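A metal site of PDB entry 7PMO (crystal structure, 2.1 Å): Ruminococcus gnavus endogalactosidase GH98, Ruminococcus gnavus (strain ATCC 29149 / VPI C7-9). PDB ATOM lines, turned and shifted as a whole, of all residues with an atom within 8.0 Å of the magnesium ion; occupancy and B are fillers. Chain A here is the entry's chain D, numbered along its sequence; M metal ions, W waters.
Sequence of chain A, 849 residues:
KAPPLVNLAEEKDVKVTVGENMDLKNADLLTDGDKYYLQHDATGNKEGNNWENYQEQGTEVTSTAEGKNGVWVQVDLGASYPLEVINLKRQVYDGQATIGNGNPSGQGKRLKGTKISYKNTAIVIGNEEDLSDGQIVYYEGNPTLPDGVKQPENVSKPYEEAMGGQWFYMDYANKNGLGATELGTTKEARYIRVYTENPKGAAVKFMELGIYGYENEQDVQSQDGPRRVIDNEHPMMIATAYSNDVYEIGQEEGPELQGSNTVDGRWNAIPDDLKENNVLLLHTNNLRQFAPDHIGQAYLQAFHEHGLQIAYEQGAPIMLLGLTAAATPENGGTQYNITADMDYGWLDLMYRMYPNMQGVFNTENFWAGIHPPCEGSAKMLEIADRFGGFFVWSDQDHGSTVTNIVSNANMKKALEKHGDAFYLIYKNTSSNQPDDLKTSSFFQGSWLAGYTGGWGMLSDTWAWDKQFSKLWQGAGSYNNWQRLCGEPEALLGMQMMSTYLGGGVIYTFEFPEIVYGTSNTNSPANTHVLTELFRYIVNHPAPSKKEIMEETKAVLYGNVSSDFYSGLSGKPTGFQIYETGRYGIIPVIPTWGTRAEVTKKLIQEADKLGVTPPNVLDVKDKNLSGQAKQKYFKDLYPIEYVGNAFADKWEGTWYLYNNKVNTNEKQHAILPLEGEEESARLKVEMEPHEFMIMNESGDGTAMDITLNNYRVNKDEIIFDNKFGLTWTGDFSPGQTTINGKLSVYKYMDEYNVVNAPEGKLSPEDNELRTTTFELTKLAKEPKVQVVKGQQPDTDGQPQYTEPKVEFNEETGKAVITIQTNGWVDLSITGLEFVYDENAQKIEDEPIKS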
ATOM      1  N   HIS A 528       4.373   6.683  -7.450  1.00  0.00           N
ATOM      2  CA  HIS A 528       4.286   7.488  -6.201  1.00  0.00           C
ATOM      3  C   HIS A 528       3.253   6.923  -5.223  1.00  0.00           C
ATOM      4  O   HIS A 528       3.287   7.372  -4.074  1.00  0.00           O
ATOM      5  CB  HIS A 528       4.014   8.959  -6.552  1.00  0.00           C
ATOM      6  CG  HIS A 528       5.083   9.591  -7.373  1.00  0.00           C
ATOM      7  ND1 HIS A 528       6.422   9.516  -7.029  1.00  0.00           N
ATOM      8  CD2 HIS A 528       5.026  10.326  -8.510  1.00  0.00           C
ATOM      9  CE1 HIS A 528       7.144  10.187  -7.915  1.00  0.00           C
ATOM     10  NE2 HIS A 528       6.310  10.692  -8.836  1.00  0.00           N
ATOM     11  N   TYR A 710      -0.757  11.916  -2.655  1.00  0.00           N
ATOM     12  CA  TYR A 710      -0.423  12.172  -4.078  1.00  0.00           C
ATOM     13  C   TYR A 710      -1.689  12.301  -4.914  1.00  0.00           C
ATOM     14  O   TYR A 710      -2.514  11.364  -4.931  1.00  0.00           O
ATOM     15  CB  TYR A 710       0.457  11.068  -4.671  1.00  0.00           C
ATOM     16  CG  TYR A 710       1.007  11.454  -6.023  1.00  0.00           C
ATOM     17  CD1 TYR A 710       1.857  12.540  -6.141  1.00  0.00           C
ATOM     18  CD2 TYR A 710       0.640  10.782  -7.179  1.00  0.00           C
ATOM     19  CE1 TYR A 710       2.343  12.935  -7.376  1.00  0.00           C
ATOM     20  CE2 TYR A 710       1.120  11.155  -8.413  1.00  0.00           C
ATOM     21  CZ  TYR A 710       1.963  12.243  -8.511  1.00  0.00           C
ATOM     22  OH  TYR A 710       2.472  12.641  -9.712  1.00  0.00           O
ATOM     23  N   SER A 762       5.874  17.275 -16.916  1.00  0.00           N
ATOM     24  CA  SER A 762       5.829  16.707 -15.542  1.00  0.00           C
ATOM     25  C   SER A 762       4.363  16.612 -15.130  1.00  0.00           C
ATOM     26  O   SER A 762       3.530  17.386 -15.603  1.00  0.00           O
ATOM     27  CB  SER A 762       6.620  17.540 -14.553  1.00  0.00           C
ATOM     28  OG  SER A 762       7.990  17.624 -14.939  1.00  0.00           O
ATOM     29  N   PRO A 763       4.007  15.685 -14.215  1.00  0.00           N
ATOM     30  CA  PRO A 763       2.621  15.588 -13.748  1.00  0.00           C
ATOM     31  C   PRO A 763       2.243  16.892 -13.044  1.00  0.00           C
ATOM     32  O   PRO A 763       3.098  17.523 -12.449  1.00  0.00           O
ATOM     33  CB  PRO A 763       2.625  14.398 -12.788  1.00  0.00           C
ATOM     34  CG  PRO A 763       3.879  13.625 -13.162  1.00  0.00           C
ATOM     35  CD  PRO A 763       4.880  14.686 -13.600  1.00  0.00           C
ATOM     36  N   GLU A 764       0.970  17.248 -13.152  1.00  0.00           N
ATOM     37  CA  GLU A 764       0.383  18.466 -12.544  1.00  0.00           C
ATOM     38  C   GLU A 764       0.051  18.135 -11.082  1.00  0.00           C
ATOM     39  O   GLU A 764      -1.137  18.008 -10.768  1.00  0.00           O
ATOM     40  CB  GLU A 764      -0.820  18.901 -13.364  1.00  0.00           C
ATOM     41  CG  GLU A 764      -1.278  20.313 -13.063  1.00  0.00           C
ATOM     42  CD  GLU A 764      -0.353  21.364 -13.651  1.00  0.00           C
ATOM     43  OE1 GLU A 764      -0.514  21.663 -14.850  1.00  0.00           O
ATOM     44  OE2 GLU A 764       0.538  21.821 -12.929  1.00  0.00           O
ATOM     45  N   ASP A 765       1.078  18.060 -10.227  1.00  0.00           N
ATOM     46  CA  ASP A 765       0.985  17.519  -8.849  1.00  0.00           C
ATOM     47  C   ASP A 765       1.650  18.468  -7.840  1.00  0.00           C
ATOM     48  O   ASP A 765       2.104  17.971  -6.791  1.00  0.00           O
ATOM     49  CB  ASP A 765       1.634  16.122  -8.802  1.00  0.00           C
ATOM     50  CG  ASP A 765       3.108  16.142  -9.197  1.00  0.00           C
ATOM     51  OD1 ASP A 765       3.734  17.233  -9.102  1.00  0.00           O
ATOM     52  OD2 ASP A 765       3.615  15.068  -9.592  1.00  0.00           O
ATOM     53  N   ASN A 766       1.718  19.768  -8.148  1.00  0.00           N
ATOM     54  CA  ASN A 766       2.571  20.730  -7.404  1.00  0.00           C
ATOM     55  C   ASN A 766       1.768  21.556  -6.399  1.00  0.00           C
ATOM     56  O   ASN A 766       2.408  22.231  -5.583  1.00  0.00           O
ATOM     57  CB  ASN A 766       3.372  21.600  -8.383  1.00  0.00           C
ATOM     58  CG  ASN A 766       4.353  20.772  -9.190  1.00  0.00           C
ATOM     59  OD1 ASN A 766       4.900  19.796  -8.686  1.00  0.00           O
ATOM     60  ND2 ASN A 766       4.589  21.144 -10.432  1.00  0.00           N
ATOM     61  N   GLU A 767       0.425  21.510  -6.437  1.00  0.00           N
ATOM     62  CA  GLU A 767      -0.459  22.154  -5.425  1.00  0.00           C
ATOM     63  C   GLU A 767      -0.453  21.295  -4.152  1.00  0.00           C
ATOM     64  O   GLU A 767      -0.995  20.151  -4.177  1.00  0.00           O
ATOM     65  CB  GLU A 767      -1.899  22.313  -5.902  1.00  0.00           C
ATOM     66  CG  GLU A 767      -2.079  23.237  -7.079  1.00  0.00           C
ATOM     67  CD  GLU A 767      -3.472  23.147  -7.675  1.00  0.00           C
ATOM     68  OE1 GLU A 767      -3.704  22.227  -8.522  1.00  0.00           O
ATOM     69  OE2 GLU A 767      -4.353  23.949  -7.266  1.00  0.00           O
ATOM     70  N   LEU A 768       0.102  21.821  -3.063  1.00  0.00           N
ATOM     71  CA  LEU A 768       0.306  21.104  -1.790  1.00  0.00           C
ATOM     72  C   LEU A 768      -0.940  21.304  -0.923  1.00  0.00           C
ATOM     73  O   LEU A 768      -1.604  22.324  -1.064  1.00  0.00           O
ATOM     74  CB  LEU A 768       1.562  21.637  -1.109  1.00  0.00           C
ATOM     75  CG  LEU A 768       2.810  21.696  -1.982  1.00  0.00           C
ATOM     76  CD1 LEU A 768       4.012  22.184  -1.192  1.00  0.00           C
ATOM     77  CD2 LEU A 768       3.102  20.346  -2.614  1.00  0.00           C
ATOM     78  N   GLN A 790       9.268  12.544  -1.052  1.00  0.00           N
ATOM     79  CA  GLN A 790       9.110  12.452  -2.529  1.00  0.00           C
ATOM     80  C   GLN A 790       9.828  13.648  -3.163  1.00  0.00           C
ATOM     81  O   GLN A 790       9.599  14.789  -2.744  1.00  0.00           O
ATOM     82  CB  GLN A 790       7.625  12.402  -2.926  1.00  0.00           C
ATOM     83  CG  GLN A 790       7.412  12.235  -4.422  1.00  0.00           C
ATOM     84  CD  GLN A 790       5.948  12.079  -4.762  1.00  0.00           C
ATOM     85  OE1 GLN A 790       5.164  11.553  -3.979  1.00  0.00           O
ATOM     86  NE2 GLN A 790       5.554  12.541  -5.941  1.00  0.00           N
ATOM     87  N   GLN A 791      10.691  13.343  -4.134  1.00  0.00           N
ATOM     88  CA  GLN A 791      11.604  14.300  -4.802  1.00  0.00           C
ATOM     89  C   GLN A 791      10.881  14.953  -5.974  1.00  0.00           C
ATOM     90  O   GLN A 791       9.905  14.400  -6.492  1.00  0.00           O
ATOM     91  CB  GLN A 791      12.881  13.570  -5.252  1.00  0.00           C
ATOM     92  CG  GLN A 791      13.703  13.044  -4.091  1.00  0.00           C
ATOM     93  CD  GLN A 791      13.963  14.130  -3.082  1.00  0.00           C
ATOM     94  OE1 GLN A 791      13.441  14.136  -1.961  1.00  0.00           O
ATOM     95  NE2 GLN A 791      14.741  15.106  -3.495  1.00  0.00           N
ATOM     96  N   PRO A 792      11.322  16.154  -6.428  1.00  0.00           N
ATOM     97  CA  PRO A 792      10.674  16.835  -7.536  1.00  0.00           C
ATOM     98  C   PRO A 792      10.806  16.046  -8.853  1.00  0.00           C
ATOM     99  O   PRO A 792      11.768  15.305  -9.007  1.00  0.00           O
ATOM    100  CB  PRO A 792      11.457  18.156  -7.665  1.00  0.00           C
ATOM    101  CG  PRO A 792      12.151  18.339  -6.327  1.00  0.00           C
ATOM    102  CD  PRO A 792      12.462  16.919  -5.882  1.00  0.00           C
ATOM    103  N   ASP A 793       9.851  16.259  -9.760  1.00  0.00           N
ATOM    104  CA  ASP A 793       9.983  15.879 -11.194  1.00  0.00           C
ATOM    105  C   ASP A 793      10.986  16.844 -11.833  1.00  0.00           C
ATOM    106  O   ASP A 793      11.575  17.662 -11.117  1.00  0.00           O
ATOM    107  CB  ASP A 793       8.628  15.916 -11.884  1.00  0.00           C
ATOM    108  CG  ASP A 793       8.489  14.835 -12.934  1.00  0.00           C
ATOM    109  OD1 ASP A 793       8.205  13.675 -12.538  1.00  0.00           O
ATOM    110  OD2 ASP A 793       8.722  15.144 -14.110  1.00  0.00           O
ATOM    111  N   THR A 794      11.163  16.764 -13.159  1.00  0.00           N
ATOM    112  CA  THR A 794      12.149  17.533 -13.944  1.00  0.00           C
ATOM    113  C   THR A 794      11.782  19.024 -13.955  1.00  0.00           C
ATOM    114  O   THR A 794      12.665  19.825 -14.329  1.00  0.00           O
ATOM    115  CB  THR A 794      12.279  16.928 -15.347  1.00  0.00           C
ATOM    116  OG1 THR A 794      10.965  16.827 -15.893  1.00  0.00           O
ATOM    117  CG2 THR A 794      12.938  15.570 -15.338  1.00  0.00           C
ATOM    118  N   ASP A 795      10.564  19.409 -13.566  1.00  0.00           N
ATOM    119  CA  ASP A 795      10.150  20.843 -13.468  1.00  0.00           C
ATOM    120  C   ASP A 795      10.719  21.479 -12.189  1.00  0.00           C
ATOM    121  O   ASP A 795      10.558  22.691 -12.013  1.00  0.00           O
ATOM    122  CB  ASP A 795       8.623  21.002 -13.540  1.00  0.00           C
ATOM    123  CG  ASP A 795       7.837  20.301 -12.427  1.00  0.00           C
ATOM    124  OD1 ASP A 795       8.475  19.749 -11.500  1.00  0.00           O
ATOM    125  OD2 ASP A 795       6.609  20.317 -12.508  1.00  0.00           O
ATOM    126  N   GLY A 796      11.315  20.674 -11.303  1.00  0.00           N
ATOM    127  CA  GLY A 796      12.075  21.144 -10.121  1.00  0.00           C
ATOM    128  C   GLY A 796      11.186  21.592  -8.973  1.00  0.00           C
ATOM    129  O   GLY A 796      11.743  22.138  -8.025  1.00  0.00           O
ATOM    130  N   GLN A 797       9.871  21.368  -9.040  1.00  0.00           N
ATOM    131  CA  GLN A 797       8.906  21.866  -8.028  1.00  0.00           C
ATOM    132  C   GLN A 797       8.817  20.882  -6.868  1.00  0.00           C
ATOM    133  O   GLN A 797       8.685  19.671  -7.069  1.00  0.00           O
ATOM    134  CB  GLN A 797       7.526  22.096  -8.648  1.00  0.00           C
ATOM    135  CG  GLN A 797       7.541  23.048  -9.839  1.00  0.00           C
ATOM    136  CD  GLN A 797       7.931  24.435  -9.415  1.00  0.00           C
ATOM    137  OE1 GLN A 797       7.406  24.966  -8.445  1.00  0.00           O
ATOM    138  NE2 GLN A 797       8.874  25.032 -10.128  1.00  0.00           N
ATOM    139  N   PRO A 798       8.893  21.373  -5.605  1.00  0.00           N
ATOM    140  CA  PRO A 798       8.839  20.500  -4.431  1.00  0.00           C
ATOM    141  C   PRO A 798       7.479  19.816  -4.234  1.00  0.00           C
ATOM    142  O   PRO A 798       6.463  20.389  -4.587  1.00  0.00           O
ATOM    143  CB  PRO A 798       9.137  21.454  -3.266  1.00  0.00           C
ATOM    144  CG  PRO A 798       8.674  22.806  -3.765  1.00  0.00           C
ATOM    145  CD  PRO A 798       9.039  22.800  -5.228  1.00  0.00           C
ATOM    146  N   GLN A 799       7.482  18.612  -3.649  1.00  0.00           N
ATOM    147  CA  GLN A 799       6.245  17.846  -3.356  1.00  0.00           C
ATOM    148  C   GLN A 799       5.936  17.949  -1.854  1.00  0.00           C
ATOM    149  O   GLN A 799       4.898  17.410  -1.455  1.00  0.00           O
ATOM    150  CB  GLN A 799       6.376  16.406  -3.847  1.00  0.00           C
ATOM    151  CG  GLN A 799       6.807  16.280  -5.309  1.00  0.00           C
ATOM    152  CD  GLN A 799       5.819  16.843  -6.314  1.00  0.00           C
ATOM    153  OE1 GLN A 799       6.189  17.376  -7.365  1.00  0.00           O
ATOM    154  NE2 GLN A 799       4.539  16.712  -6.016  1.00  0.00           N
ATOM    155  N   ASN A 821       2.125  17.042  -1.508  1.00  0.00           N
ATOM    156  CA  ASN A 821       1.401  16.357  -2.593  1.00  0.00           C
ATOM    157  C   ASN A 821       2.288  15.184  -3.016  1.00  0.00           C
ATOM    158  O   ASN A 821       3.150  15.375  -3.884  1.00  0.00           O
ATOM    159  CB  ASN A 821       1.042  17.295  -3.732  1.00  0.00           C
ATOM    160  CG  ASN A 821       0.057  16.661  -4.692  1.00  0.00           C
ATOM    161  OD1 ASN A 821      -0.005  15.446  -4.808  1.00  0.00           O
ATOM    162  ND2 ASN A 821      -0.713  17.480  -5.375  1.00  0.00           N
HETATM  163 MG    MG M   1       5.633  17.954  -9.276  1.00  0.00          MG
HETATM  164  O   HOH W   1       7.642  18.310  -9.338  1.00  0.00           O
HETATM  165  O   HOH W   2       6.185  15.688  -9.434  1.00  0.00           O
HETATM  166  O   HOH W   3       5.690  18.044 -11.249  1.00  0.00           O
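OD2 of Asp 765 is in hydrogen-bond range of OH of Tyr 710, 2.7 Å away. O of Asp 765 lies within hydrogen-bond range of ND2 of Asn 821, at 3.2 Å. OD2 of Asp 795 sits at hydrogen-bond distance from ND2 of Asn 766 (3.0 Å). O of Gln 797 sits close to OE1 of Gln 799 (3.4 Å). The backbone carbonyl oxygen (O) of Gln 799 is in hydrogen-bond range of the backbone NH (N) of Asn 821.
Water W3 is bound to the magnesium ion, at 2.0 Å. OD1 of Asp 765 binds the magnesium ion (2.0 Å). Water W1 binds the magnesium ion (2.0 Å). The side-chain amide oxygen (OD1) of Asn 766 binds the magnesium ion (2.1 Å). OE1 of Gln 799 is bound to the magnesium ion (2.1 Å). The magnesium ion is bound by water W2 (2.3 Å). The magnesium ion has six donor atoms within binding distance.
Water W1 lies within hydrogen-bond range of OD1 of Asp 795 (2.7 Å), O of Gln 797 (2.8 Å) and N of Asp 793 (3.0 Å). Water W3 lies within hydrogen-bond range of OD2 of Asp 795 (2.8 Å), O of Pro 763 (2.9 Å) and ND2 of Asn 766 (3.4 Å).
Of the 20 residues printed, 3 come within 4 Å of the magnesium ion.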
